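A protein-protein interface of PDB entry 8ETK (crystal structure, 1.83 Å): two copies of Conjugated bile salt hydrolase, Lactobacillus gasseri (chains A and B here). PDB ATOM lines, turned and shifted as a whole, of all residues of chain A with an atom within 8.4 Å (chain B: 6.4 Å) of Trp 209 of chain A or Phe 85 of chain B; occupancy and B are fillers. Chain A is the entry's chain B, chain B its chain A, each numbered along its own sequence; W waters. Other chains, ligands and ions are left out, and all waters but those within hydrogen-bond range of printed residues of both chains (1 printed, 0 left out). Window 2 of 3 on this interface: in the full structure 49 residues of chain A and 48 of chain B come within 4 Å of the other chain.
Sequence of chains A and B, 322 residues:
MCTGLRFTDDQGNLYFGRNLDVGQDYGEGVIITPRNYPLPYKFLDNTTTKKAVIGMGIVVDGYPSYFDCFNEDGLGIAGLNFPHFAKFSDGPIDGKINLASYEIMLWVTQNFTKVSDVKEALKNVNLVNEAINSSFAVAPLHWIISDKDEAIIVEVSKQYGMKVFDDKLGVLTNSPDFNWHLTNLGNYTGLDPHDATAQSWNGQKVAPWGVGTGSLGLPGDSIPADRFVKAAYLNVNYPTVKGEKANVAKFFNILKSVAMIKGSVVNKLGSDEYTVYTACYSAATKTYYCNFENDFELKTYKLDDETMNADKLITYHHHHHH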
ATOM      1  N   ALA A 196      -4.824  10.879   4.008  1.00  0.00           N
ATOM      2  CA  ALA A 196      -4.520   9.746   4.857  1.00  0.00           C
ATOM      3  C   ALA A 196      -5.553   9.643   5.979  1.00  0.00           C
ATOM      4  O   ALA A 196      -6.375  10.539   6.187  1.00  0.00           O
ATOM      5  CB  ALA A 196      -3.119   9.877   5.450  1.00  0.00           C
ATOM      6  N   GLN A 204       1.044   3.612  19.072  1.00  0.00           N
ATOM      7  CA  GLN A 204       0.820   5.049  19.191  1.00  0.00           C
ATOM      8  C   GLN A 204      -0.108   5.483  18.060  1.00  0.00           C
ATOM      9  O   GLN A 204       0.200   5.268  16.884  1.00  0.00           O
ATOM     10  CB  GLN A 204       2.139   5.824  19.125  1.00  0.00           C
ATOM     11  CG  GLN A 204       1.957   7.335  19.029  1.00  0.00           C
ATOM     12  CD  GLN A 204       1.365   7.902  20.308  1.00  0.00           C
ATOM     13  OE1 GLN A 204       1.833   7.589  21.409  1.00  0.00           O
ATOM     14  NE2 GLN A 204       0.315   8.717  20.176  1.00  0.00           N
ATOM     15  N   LYS A 205      -1.259   6.050  18.408  1.00  0.00           N
ATOM     16  CA  LYS A 205      -2.157   6.529  17.372  1.00  0.00           C
ATOM     17  C   LYS A 205      -1.534   7.761  16.734  1.00  0.00           C
ATOM     18  O   LYS A 205      -1.137   8.700  17.427  1.00  0.00           O
ATOM     19  CB  LYS A 205      -3.541   6.835  17.950  1.00  0.00           C
ATOM     20  CG  LYS A 205      -4.566   7.331  16.926  1.00  0.00           C
ATOM     21  CD  LYS A 205      -5.619   8.234  17.553  1.00  0.00           C
ATOM     22  CE  LYS A 205      -6.590   8.730  16.486  1.00  0.00           C
ATOM     23  NZ  LYS A 205      -7.942   9.020  17.061  1.00  0.00           N
ATOM     24  N   VAL A 206      -1.395   7.726  15.414  1.00  0.00           N
ATOM     25  CA  VAL A 206      -0.841   8.832  14.633  1.00  0.00           C
ATOM     26  C   VAL A 206      -1.867   9.099  13.541  1.00  0.00           C
ATOM     27  O   VAL A 206      -2.087   8.246  12.672  1.00  0.00           O
ATOM     28  CB  VAL A 206       0.540   8.498  14.037  1.00  0.00           C
ATOM     29  CG1 VAL A 206       1.060   9.645  13.151  1.00  0.00           C
ATOM     30  CG2 VAL A 206       1.543   8.182  15.144  1.00  0.00           C
ATOM     31  N   ALA A 207      -2.505  10.264  13.595  1.00  0.00           N
ATOM     32  CA  ALA A 207      -3.649  10.572  12.762  1.00  0.00           C
ATOM     33  C   ALA A 207      -3.548  12.005  12.255  1.00  0.00           C
ATOM     34  O   ALA A 207      -2.960  12.867  12.921  1.00  0.00           O
ATOM     35  CB  ALA A 207      -4.967  10.397  13.534  1.00  0.00           C
ATOM     36  N   PRO A 208      -4.105  12.278  11.080  1.00  0.00           N
ATOM     37  CA  PRO A 208      -4.067  13.642  10.532  1.00  0.00           C
ATOM     38  C   PRO A 208      -4.746  14.647  11.456  1.00  0.00           C
ATOM     39  O   PRO A 208      -5.768  14.357  12.085  1.00  0.00           O
ATOM     40  CB  PRO A 208      -4.821  13.510   9.199  1.00  0.00           C
ATOM     41  CG  PRO A 208      -4.674  12.069   8.812  1.00  0.00           C
ATOM     42  CD  PRO A 208      -4.662  11.299  10.127  1.00  0.00           C
ATOM     43  N   TRP A 209      -4.167  15.845  11.527  1.00  0.00           N
ATOM     44  CA  TRP A 209      -4.772  16.949  12.277  1.00  0.00           C
ATOM     45  C   TRP A 209      -5.793  17.714  11.449  1.00  0.00           C
ATOM     46  O   TRP A 209      -6.698  18.335  12.020  1.00  0.00           O
ATOM     47  CB  TRP A 209      -3.676  17.914  12.779  1.00  0.00           C
ATOM     48  CG  TRP A 209      -2.796  17.262  13.804  1.00  0.00           C
ATOM     49  CD1 TRP A 209      -1.478  16.909  13.666  1.00  0.00           C
ATOM     50  CD2 TRP A 209      -3.185  16.855  15.117  1.00  0.00           C
ATOM     51  NE1 TRP A 209      -1.029  16.311  14.822  1.00  0.00           N
ATOM     52  CE2 TRP A 209      -2.057  16.269  15.727  1.00  0.00           C
ATOM     53  CE3 TRP A 209      -4.381  16.936  15.841  1.00  0.00           C
ATOM     54  CZ2 TRP A 209      -2.091  15.755  17.029  1.00  0.00           C
ATOM     55  CZ3 TRP A 209      -4.406  16.432  17.140  1.00  0.00           C
ATOM     56  CH2 TRP A 209      -3.271  15.856  17.715  1.00  0.00           C
ATOM     57  N   GLY A 210      -5.662  17.678  10.124  1.00  0.00           N
ATOM     58  CA  GLY A 210      -6.581  18.326   9.201  1.00  0.00           C
ATOM     59  C   GLY A 210      -6.423  17.662   7.849  1.00  0.00           C
ATOM     60  O   GLY A 210      -5.614  16.747   7.683  1.00  0.00           O
ATOM     61  N   VAL A 211      -7.208  18.134   6.871  1.00  0.00           N
ATOM     62  CA  VAL A 211      -7.166  17.562   5.528  1.00  0.00           C
ATOM     63  C   VAL A 211      -5.917  18.041   4.781  1.00  0.00           C
ATOM     64  O   VAL A 211      -5.278  19.042   5.138  1.00  0.00           O
ATOM     65  CB  VAL A 211      -8.454  17.904   4.745  1.00  0.00           C
ATOM     66  CG1 VAL A 211      -9.714  17.422   5.519  1.00  0.00           C
ATOM     67  CG2 VAL A 211      -8.535  19.410   4.437  1.00  0.00           C
ATOM     68  N   GLY A 212      -5.570  17.316   3.711  1.00  0.00           N
ATOM     69  CA  GLY A 212      -4.409  17.633   2.888  1.00  0.00           C
ATOM     70  C   GLY A 212      -3.238  16.674   2.988  1.00  0.00           C
ATOM     71  O   GLY A 212      -2.245  16.859   2.272  1.00  0.00           O
ATOM     72  N   THR A 213      -3.308  15.641   3.836  1.00  0.00           N
ATOM     73  CA  THR A 213      -2.111  14.869   4.138  1.00  0.00           C
ATOM     74  C   THR A 213      -1.605  14.043   2.966  1.00  0.00           C
ATOM     75  O   THR A 213      -0.420  13.709   2.947  1.00  0.00           O
ATOM     76  CB  THR A 213      -2.371  13.930   5.324  1.00  0.00           C
ATOM     77  OG1 THR A 213      -3.615  13.256   5.102  1.00  0.00           O
ATOM     78  CG2 THR A 213      -2.476  14.742   6.605  1.00  0.00           C
ATOM     79  N   PHE B  82     -10.781  23.902  14.750  1.00  0.00           N
ATOM     80  CA  PHE B  82      -9.709  23.488  15.651  1.00  0.00           C
ATOM     81  C   PHE B  82      -9.978  22.040  16.075  1.00  0.00           C
ATOM     82  O   PHE B  82     -10.062  21.732  17.268  1.00  0.00           O
ATOM     83  CB  PHE B  82      -9.697  24.455  16.836  1.00  0.00           C
ATOM     84  CG  PHE B  82      -8.487  24.377  17.757  1.00  0.00           C
ATOM     85  CD1 PHE B  82      -7.223  24.017  17.303  1.00  0.00           C
ATOM     86  CD2 PHE B  82      -8.639  24.715  19.104  1.00  0.00           C
ATOM     87  CE1 PHE B  82      -6.136  23.982  18.181  1.00  0.00           C
ATOM     88  CE2 PHE B  82      -7.558  24.681  20.002  1.00  0.00           C
ATOM     89  CZ  PHE B  82      -6.305  24.315  19.544  1.00  0.00           C
ATOM     90  N   PRO B  83     -10.157  21.126  15.110  1.00  0.00           N
ATOM     91  CA  PRO B  83     -10.605  19.770  15.458  1.00  0.00           C
ATOM     92  C   PRO B  83      -9.555  19.007  16.246  1.00  0.00           C
ATOM     93  O   PRO B  83      -8.346  19.260  16.151  1.00  0.00           O
ATOM     94  CB  PRO B  83     -10.844  19.108  14.094  1.00  0.00           C
ATOM     95  CG  PRO B  83      -9.844  19.767  13.194  1.00  0.00           C
ATOM     96  CD  PRO B  83      -9.808  21.225  13.674  1.00  0.00           C
ATOM     97  N   HIS B  84     -10.038  18.047  17.029  1.00  0.00           N
ATOM     98  CA  HIS B  84      -9.215  17.199  17.886  1.00  0.00           C
ATOM     99  C   HIS B  84      -8.582  17.974  19.029  1.00  0.00           C
ATOM    100  O   HIS B  84      -7.734  17.425  19.742  1.00  0.00           O
ATOM    101  CB  HIS B  84      -8.115  16.467  17.101  1.00  0.00           C
ATOM    102  CG  HIS B  84      -8.568  15.960  15.769  1.00  0.00           C
ATOM    103  ND1 HIS B  84      -9.476  14.930  15.633  1.00  0.00           N
ATOM    104  CD2 HIS B  84      -8.269  16.367  14.511  1.00  0.00           C
ATOM    105  CE1 HIS B  84      -9.697  14.706  14.349  1.00  0.00           C
ATOM    106  NE2 HIS B  84      -8.980  15.569  13.647  1.00  0.00           N
ATOM    107  N   PHE B  85      -8.967  19.240  19.225  1.00  0.00           N
ATOM    108  CA  PHE B  85      -8.398  20.072  20.277  1.00  0.00           C
ATOM    109  C   PHE B  85      -9.494  20.827  21.005  1.00  0.00           C
ATOM    110  O   PHE B  85      -9.587  20.763  22.236  1.00  0.00           O
ATOM    111  CB  PHE B  85      -7.412  21.091  19.705  1.00  0.00           C
ATOM    112  CG  PHE B  85      -5.993  20.620  19.666  1.00  0.00           C
ATOM    113  CD1 PHE B  85      -5.529  19.885  18.582  1.00  0.00           C
ATOM    114  CD2 PHE B  85      -5.111  20.953  20.679  1.00  0.00           C
ATOM    115  CE1 PHE B  85      -4.222  19.459  18.527  1.00  0.00           C
ATOM    116  CE2 PHE B  85      -3.789  20.529  20.628  1.00  0.00           C
ATOM    117  CZ  PHE B  85      -3.349  19.782  19.544  1.00  0.00           C
ATOM    118  N   ALA B  86     -10.317  21.563  20.250  1.00  0.00           N
ATOM    119  CA  ALA B  86     -11.299  22.450  20.866  1.00  0.00           C
ATOM    120  C   ALA B  86     -12.176  21.684  21.846  1.00  0.00           C
ATOM    121  O   ALA B  86     -12.742  20.646  21.497  1.00  0.00           O
ATOM    122  CB  ALA B  86     -12.179  23.089  19.789  1.00  0.00           C
ATOM    123  N   LYS B  87     -12.294  22.204  23.069  1.00  0.00           N
ATOM    124  CA  LYS B  87     -13.199  21.623  24.058  1.00  0.00           C
ATOM    125  C   LYS B  87     -13.621  22.712  25.031  1.00  0.00           C
ATOM    126  O   LYS B  87     -12.774  23.307  25.699  1.00  0.00           O
ATOM    127  CB  LYS B  87     -12.545  20.468  24.817  1.00  0.00           C
ATOM    128  CG  LYS B  87     -13.571  19.574  25.548  1.00  0.00           C
ATOM    129  CD  LYS B  87     -13.518  19.841  27.049  1.00  0.00           C
ATOM    130  CE  LYS B  87     -14.517  18.977  27.819  1.00  0.00           C
ATOM    131  NZ  LYS B  87     -15.381  19.782  28.738  1.00  0.00           N
ATOM    132  N   PRO B 140     -16.198  22.997  16.691  1.00  0.00           N
ATOM    133  CA  PRO B 140     -14.953  23.025  17.486  1.00  0.00           C
ATOM    134  C   PRO B 140     -13.983  24.104  17.020  1.00  0.00           C
ATOM    135  O   PRO B 140     -12.952  23.841  16.399  1.00  0.00           O
ATOM    136  CB  PRO B 140     -14.394  21.616  17.257  1.00  0.00           C
ATOM    137  CG  PRO B 140     -14.822  21.273  15.836  1.00  0.00           C
ATOM    138  CD  PRO B 140     -16.142  22.006  15.597  1.00  0.00           C
ATOM    139  N   VAL B 156      -9.354  27.276  23.245  1.00  0.00           N
ATOM    140  CA  VAL B 156      -9.747  26.538  24.446  1.00  0.00           C
ATOM    141  C   VAL B 156      -9.715  25.060  24.100  1.00  0.00           C
ATOM    142  O   VAL B 156     -10.511  24.592  23.276  1.00  0.00           O
ATOM    143  CB  VAL B 156     -11.135  26.949  24.959  1.00  0.00           C
ATOM    144  CG1 VAL B 156     -11.387  26.390  26.377  1.00  0.00           C
ATOM    145  CG2 VAL B 156     -11.259  28.477  24.934  1.00  0.00           C
ATOM    146  N   SER B 157      -8.820  24.322  24.735  1.00  0.00           N
ATOM    147  CA  SER B 157      -8.596  22.949  24.331  1.00  0.00           C
ATOM    148  C   SER B 157      -8.725  22.022  25.524  1.00  0.00           C
ATOM    149  O   SER B 157      -8.498  22.417  26.669  1.00  0.00           O
ATOM    150  CB  SER B 157      -7.225  22.783  23.685  1.00  0.00           C
ATOM    151  OG  SER B 157      -6.195  23.123  24.593  1.00  0.00           O
ATOM    152  N   LYS B 158      -9.107  20.779  25.239  1.00  0.00           N
ATOM    153  CA  LYS B 158      -9.036  19.774  26.285  1.00  0.00           C
ATOM    154  C   LYS B 158      -7.607  19.624  26.776  1.00  0.00           C
ATOM    155  O   LYS B 158      -7.393  19.349  27.955  1.00  0.00           O
ATOM    156  CB  LYS B 158      -9.612  18.444  25.790  1.00  0.00           C
ATOM    157  CG  LYS B 158      -8.858  17.799  24.640  1.00  0.00           C
ATOM    158  CD  LYS B 158      -9.437  16.419  24.317  1.00  0.00           C
ATOM    159  CE  LYS B 158      -9.590  16.204  22.821  1.00  0.00           C
ATOM    160  NZ  LYS B 158      -9.045  14.879  22.437  1.00  0.00           N
ATOM    161  N   GLN B 159      -6.620  19.891  25.909  1.00  0.00           N
ATOM    162  CA  GLN B 159      -5.215  19.694  26.260  1.00  0.00           C
ATOM    163  C   GLN B 159      -4.650  20.811  27.135  1.00  0.00           C
ATOM    164  O   GLN B 159      -3.882  20.532  28.061  1.00  0.00           O
ATOM    165  CB  GLN B 159      -4.370  19.557  24.989  1.00  0.00           C
ATOM    166  CG  GLN B 159      -4.641  18.303  24.156  1.00  0.00           C
ATOM    167  CD  GLN B 159      -5.690  18.523  23.076  1.00  0.00           C
ATOM    168  OE1 GLN B 159      -6.510  19.443  23.166  1.00  0.00           O
ATOM    169  NE2 GLN B 159      -5.658  17.684  22.035  1.00  0.00           N
ATOM    170  N   TYR B 160      -4.971  22.086  26.848  1.00  0.00           N
ATOM    171  CA  TYR B 160      -4.304  23.203  27.515  1.00  0.00           C
ATOM    172  C   TYR B 160      -5.222  24.218  28.194  1.00  0.00           C
ATOM    173  O   TYR B 160      -4.715  25.223  28.704  1.00  0.00           O
ATOM    174  CB  TYR B 160      -3.400  23.962  26.525  1.00  0.00           C
ATOM    175  CG  TYR B 160      -2.447  23.055  25.796  1.00  0.00           C
ATOM    176  CD1 TYR B 160      -1.503  22.303  26.498  1.00  0.00           C
ATOM    177  CD2 TYR B 160      -2.497  22.924  24.415  1.00  0.00           C
ATOM    178  CE1 TYR B 160      -0.630  21.453  25.839  1.00  0.00           C
ATOM    179  CE2 TYR B 160      -1.624  22.083  23.745  1.00  0.00           C
ATOM    180  CZ  TYR B 160      -0.694  21.348  24.458  1.00  0.00           C
ATOM    181  OH  TYR B 160       0.171  20.505  23.785  1.00  0.00           O
ATOM    182  N   ASN B 174      -5.395  25.845  11.104  1.00  0.00           N
ATOM    183  CA  ASN B 174      -6.198  24.904  11.878  1.00  0.00           C
ATOM    184  C   ASN B 174      -5.293  24.129  12.819  1.00  0.00           C
ATOM    185  O   ASN B 174      -4.293  24.678  13.298  1.00  0.00           O
ATOM    186  CB  ASN B 174      -6.973  23.974  10.943  1.00  0.00           C
ATOM    187  CG  ASN B 174      -7.813  24.745   9.930  1.00  0.00           C
ATOM    188  OD1 ASN B 174      -7.485  24.802   8.742  1.00  0.00           O
ATOM    189  ND2 ASN B 174      -8.918  25.325  10.396  1.00  0.00           N
ATOM    190  N   SER B 175      -5.630  22.867  13.109  1.00  0.00           N
ATOM    191  CA  SER B 175      -4.915  22.161  14.170  1.00  0.00           C
ATOM    192  C   SER B 175      -3.520  21.753  13.692  1.00  0.00           C
ATOM    193  O   SER B 175      -3.295  21.548  12.492  1.00  0.00           O
ATOM    194  CB  SER B 175      -5.702  20.924  14.609  1.00  0.00           C
ATOM    195  OG  SER B 175      -6.941  21.301  15.194  1.00  0.00           O
ATOM    196  N   PRO B 176      -2.565  21.613  14.611  1.00  0.00           N
ATOM    197  CA  PRO B 176      -2.718  21.723  16.081  1.00  0.00           C
ATOM    198  C   PRO B 176      -2.706  23.145  16.660  1.00  0.00           C
ATOM    199  O   PRO B 176      -3.009  24.133  15.986  1.00  0.00           O
ATOM    200  CB  PRO B 176      -1.541  20.882  16.608  1.00  0.00           C
ATOM    201  CG  PRO B 176      -0.506  20.891  15.526  1.00  0.00           C
ATOM    202  CD  PRO B 176      -1.219  21.165  14.207  1.00  0.00           C
ATOM    203  N   ASP B 177      -2.381  23.256  17.950  1.00  0.00           N
ATOM    204  CA  ASP B 177      -2.549  24.492  18.704  1.00  0.00           C
ATOM    205  C   ASP B 177      -1.523  25.540  18.269  1.00  0.00           C
ATOM    206  O   ASP B 177      -0.517  25.235  17.633  1.00  0.00           O
ATOM    207  CB  ASP B 177      -2.385  24.212  20.199  1.00  0.00           C
ATOM    208  CG  ASP B 177      -1.025  23.626  20.505  1.00  0.00           C
ATOM    209  OD1 ASP B 177      -0.826  22.424  20.217  1.00  0.00           O
ATOM    210  OD2 ASP B 177      -0.147  24.378  20.982  1.00  0.00           O
ATOM    211  N   TRP B 180       2.195  25.296  19.064  1.00  0.00           N
ATOM    212  CA  TRP B 180       2.828  24.275  18.228  1.00  0.00           C
ATOM    213  C   TRP B 180       3.295  24.874  16.904  1.00  0.00           C
ATOM    214  O   TRP B 180       4.444  24.673  16.488  1.00  0.00           O
ATOM    215  CB  TRP B 180       1.867  23.088  17.992  1.00  0.00           C
ATOM    216  CG  TRP B 180       2.573  21.947  17.315  1.00  0.00           C
ATOM    217  CD1 TRP B 180       3.148  20.855  17.926  1.00  0.00           C
ATOM    218  CD2 TRP B 180       2.848  21.821  15.923  1.00  0.00           C
ATOM    219  NE1 TRP B 180       3.759  20.065  16.983  1.00  0.00           N
ATOM    220  CE2 TRP B 180       3.578  20.632  15.747  1.00  0.00           C
ATOM    221  CE3 TRP B 180       2.529  22.597  14.792  1.00  0.00           C
ATOM    222  CZ2 TRP B 180       3.999  20.196  14.486  1.00  0.00           C
ATOM    223  CZ3 TRP B 180       2.945  22.172  13.549  1.00  0.00           C
ATOM    224  CH2 TRP B 180       3.681  20.982  13.403  1.00  0.00           C
ATOM    225  N   ILE B 223      -1.857  20.772   4.203  1.00  0.00           N
ATOM    226  CA  ILE B 223      -1.853  20.406   5.631  1.00  0.00           C
ATOM    227  C   ILE B 223      -1.826  21.684   6.468  1.00  0.00           C
ATOM    228  O   ILE B 223      -1.106  22.644   6.101  1.00  0.00           O
ATOM    229  CB  ILE B 223      -0.642  19.499   5.947  1.00  0.00           C
ATOM    230  CG1 ILE B 223      -0.742  18.187   5.136  1.00  0.00           C
ATOM    231  CG2 ILE B 223      -0.485  19.235   7.460  1.00  0.00           C
ATOM    232  CD1 ILE B 223       0.560  17.352   5.067  1.00  0.00           C
ATOM    233  N   PRO B 224      -2.603  21.789   7.567  1.00  0.00           N
ATOM    234  CA  PRO B 224      -2.682  23.082   8.278  1.00  0.00           C
ATOM    235  C   PRO B 224      -1.331  23.629   8.702  1.00  0.00           C
ATOM    236  O   PRO B 224      -1.115  24.840   8.596  1.00  0.00           O
ATOM    237  CB  PRO B 224      -3.569  22.770   9.491  1.00  0.00           C
ATOM    238  CG  PRO B 224      -4.454  21.644   9.023  1.00  0.00           C
ATOM    239  CD  PRO B 224      -3.537  20.799   8.136  1.00  0.00           C
HETATM  240  O   HOH W   1      -7.223  20.966  11.449  1.00  0.00           O
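O of Pro 83 of chain B lies within hydrogen-bond range of OG of Ser 175 of chain B (2.7 Å).
OG1 of Thr 213 of chain A is in hydrogen-bond range of N of Ala 196 of chain A (2.9 Å).
OE1 of Gln 159 of chain B sits close to O of Phe 85 of chain B.
The backbone carbonyl oxygen (O) of Phe 85 of chain B lies within hydrogen-bond range of the backbone NH (N) of Lys 158 of chain B (3.0 Å).
The side-chain amide nitrogen (NE2) of Gln 159 of chain B is in hydrogen-bond range of the backbone carbonyl oxygen (O) of His 84 of chain B, at 3.1 Å.
Among the printed residues, pairs that only touch across the chains: Pro 208 of chain A with His 84 of chain B (3.8 Å), Trp 209 of chain A with Pro 83 of chain B (3.7 Å), Trp 209 of chain A with His 84 of chain B (3.5 Å), Trp 209 of chain A with Phe 85 of chain B (3.3 Å), Trp 209 of chain A with Ser 175 of chain B (3.7 Å), Gly 210 of chain A with Pro 224 of chain B (3.9 Å), Val 211 of chain A with Ile 223 of chain B (3.7 Å), Val 211 of chain A with Pro 224 of chain B (3.9 Å), Gly 212 of chain A with Ile 223 of chain B (3.5 Å) and Thr 213 of chain A with Ile 223 of chain B (3.7 Å).
Trp 209 of chain A touches four residues of chain B.
Printed residues of chain B within 4 Å of Gly 210 of chain A: Pro 224.
Printed residues of chain B within 4 Å of Gly 212 of chain A: Ile 223.
Printed residues of chain A within 4 Å of Pro 83 of chain B: Trp 209.
Of the printed residues of chain A, His 84 of chain B touches Pro 208 and Trp 209.
Phe 85 of chain B touches just one residue of chain A: Trp 209.
No residue of chain A comes within 4 Å of Ala 86 of chain B.
Of the printed residues of chain A, Ser 175 of chain B touches Trp 209 (3.7 Å).
The nearest residue of chain B that does not touch Trp 209 of chain A is Pro 176 of chain B (4.2 Å).
The nearest printed residue of chain B that does not touch Val 211 of chain A is Asn 174 of chain B (6.9 Å).
Of the 11 printed residues of chain A, 6 touch a printed residue of chain B.
Hydrophobic or aromatic side chains of chain A that line the printed part of chain B: Trp 209.
Of the 19 printed residues of chain B, 6 touch a printed residue of chain A.
Along chain B the printed residues that touch a printed residue of chain A span positions 83 to 224.
Among the printed residues, no Asp or Glu carboxylate lies within 4 Å of a Lys or Arg side-chain nitrogen of the other chain.
No position is printed for both chains.
Of the 10 pairs that touch across the chains among the printed residues, none has its exchanged pair printed and touching as well.
Water W1 lies within hydrogen-bond range of the backbone carbonyl oxygen (O) of Trp 209 of chain A and the backbone NH (N) of Ser 175 of chain B.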
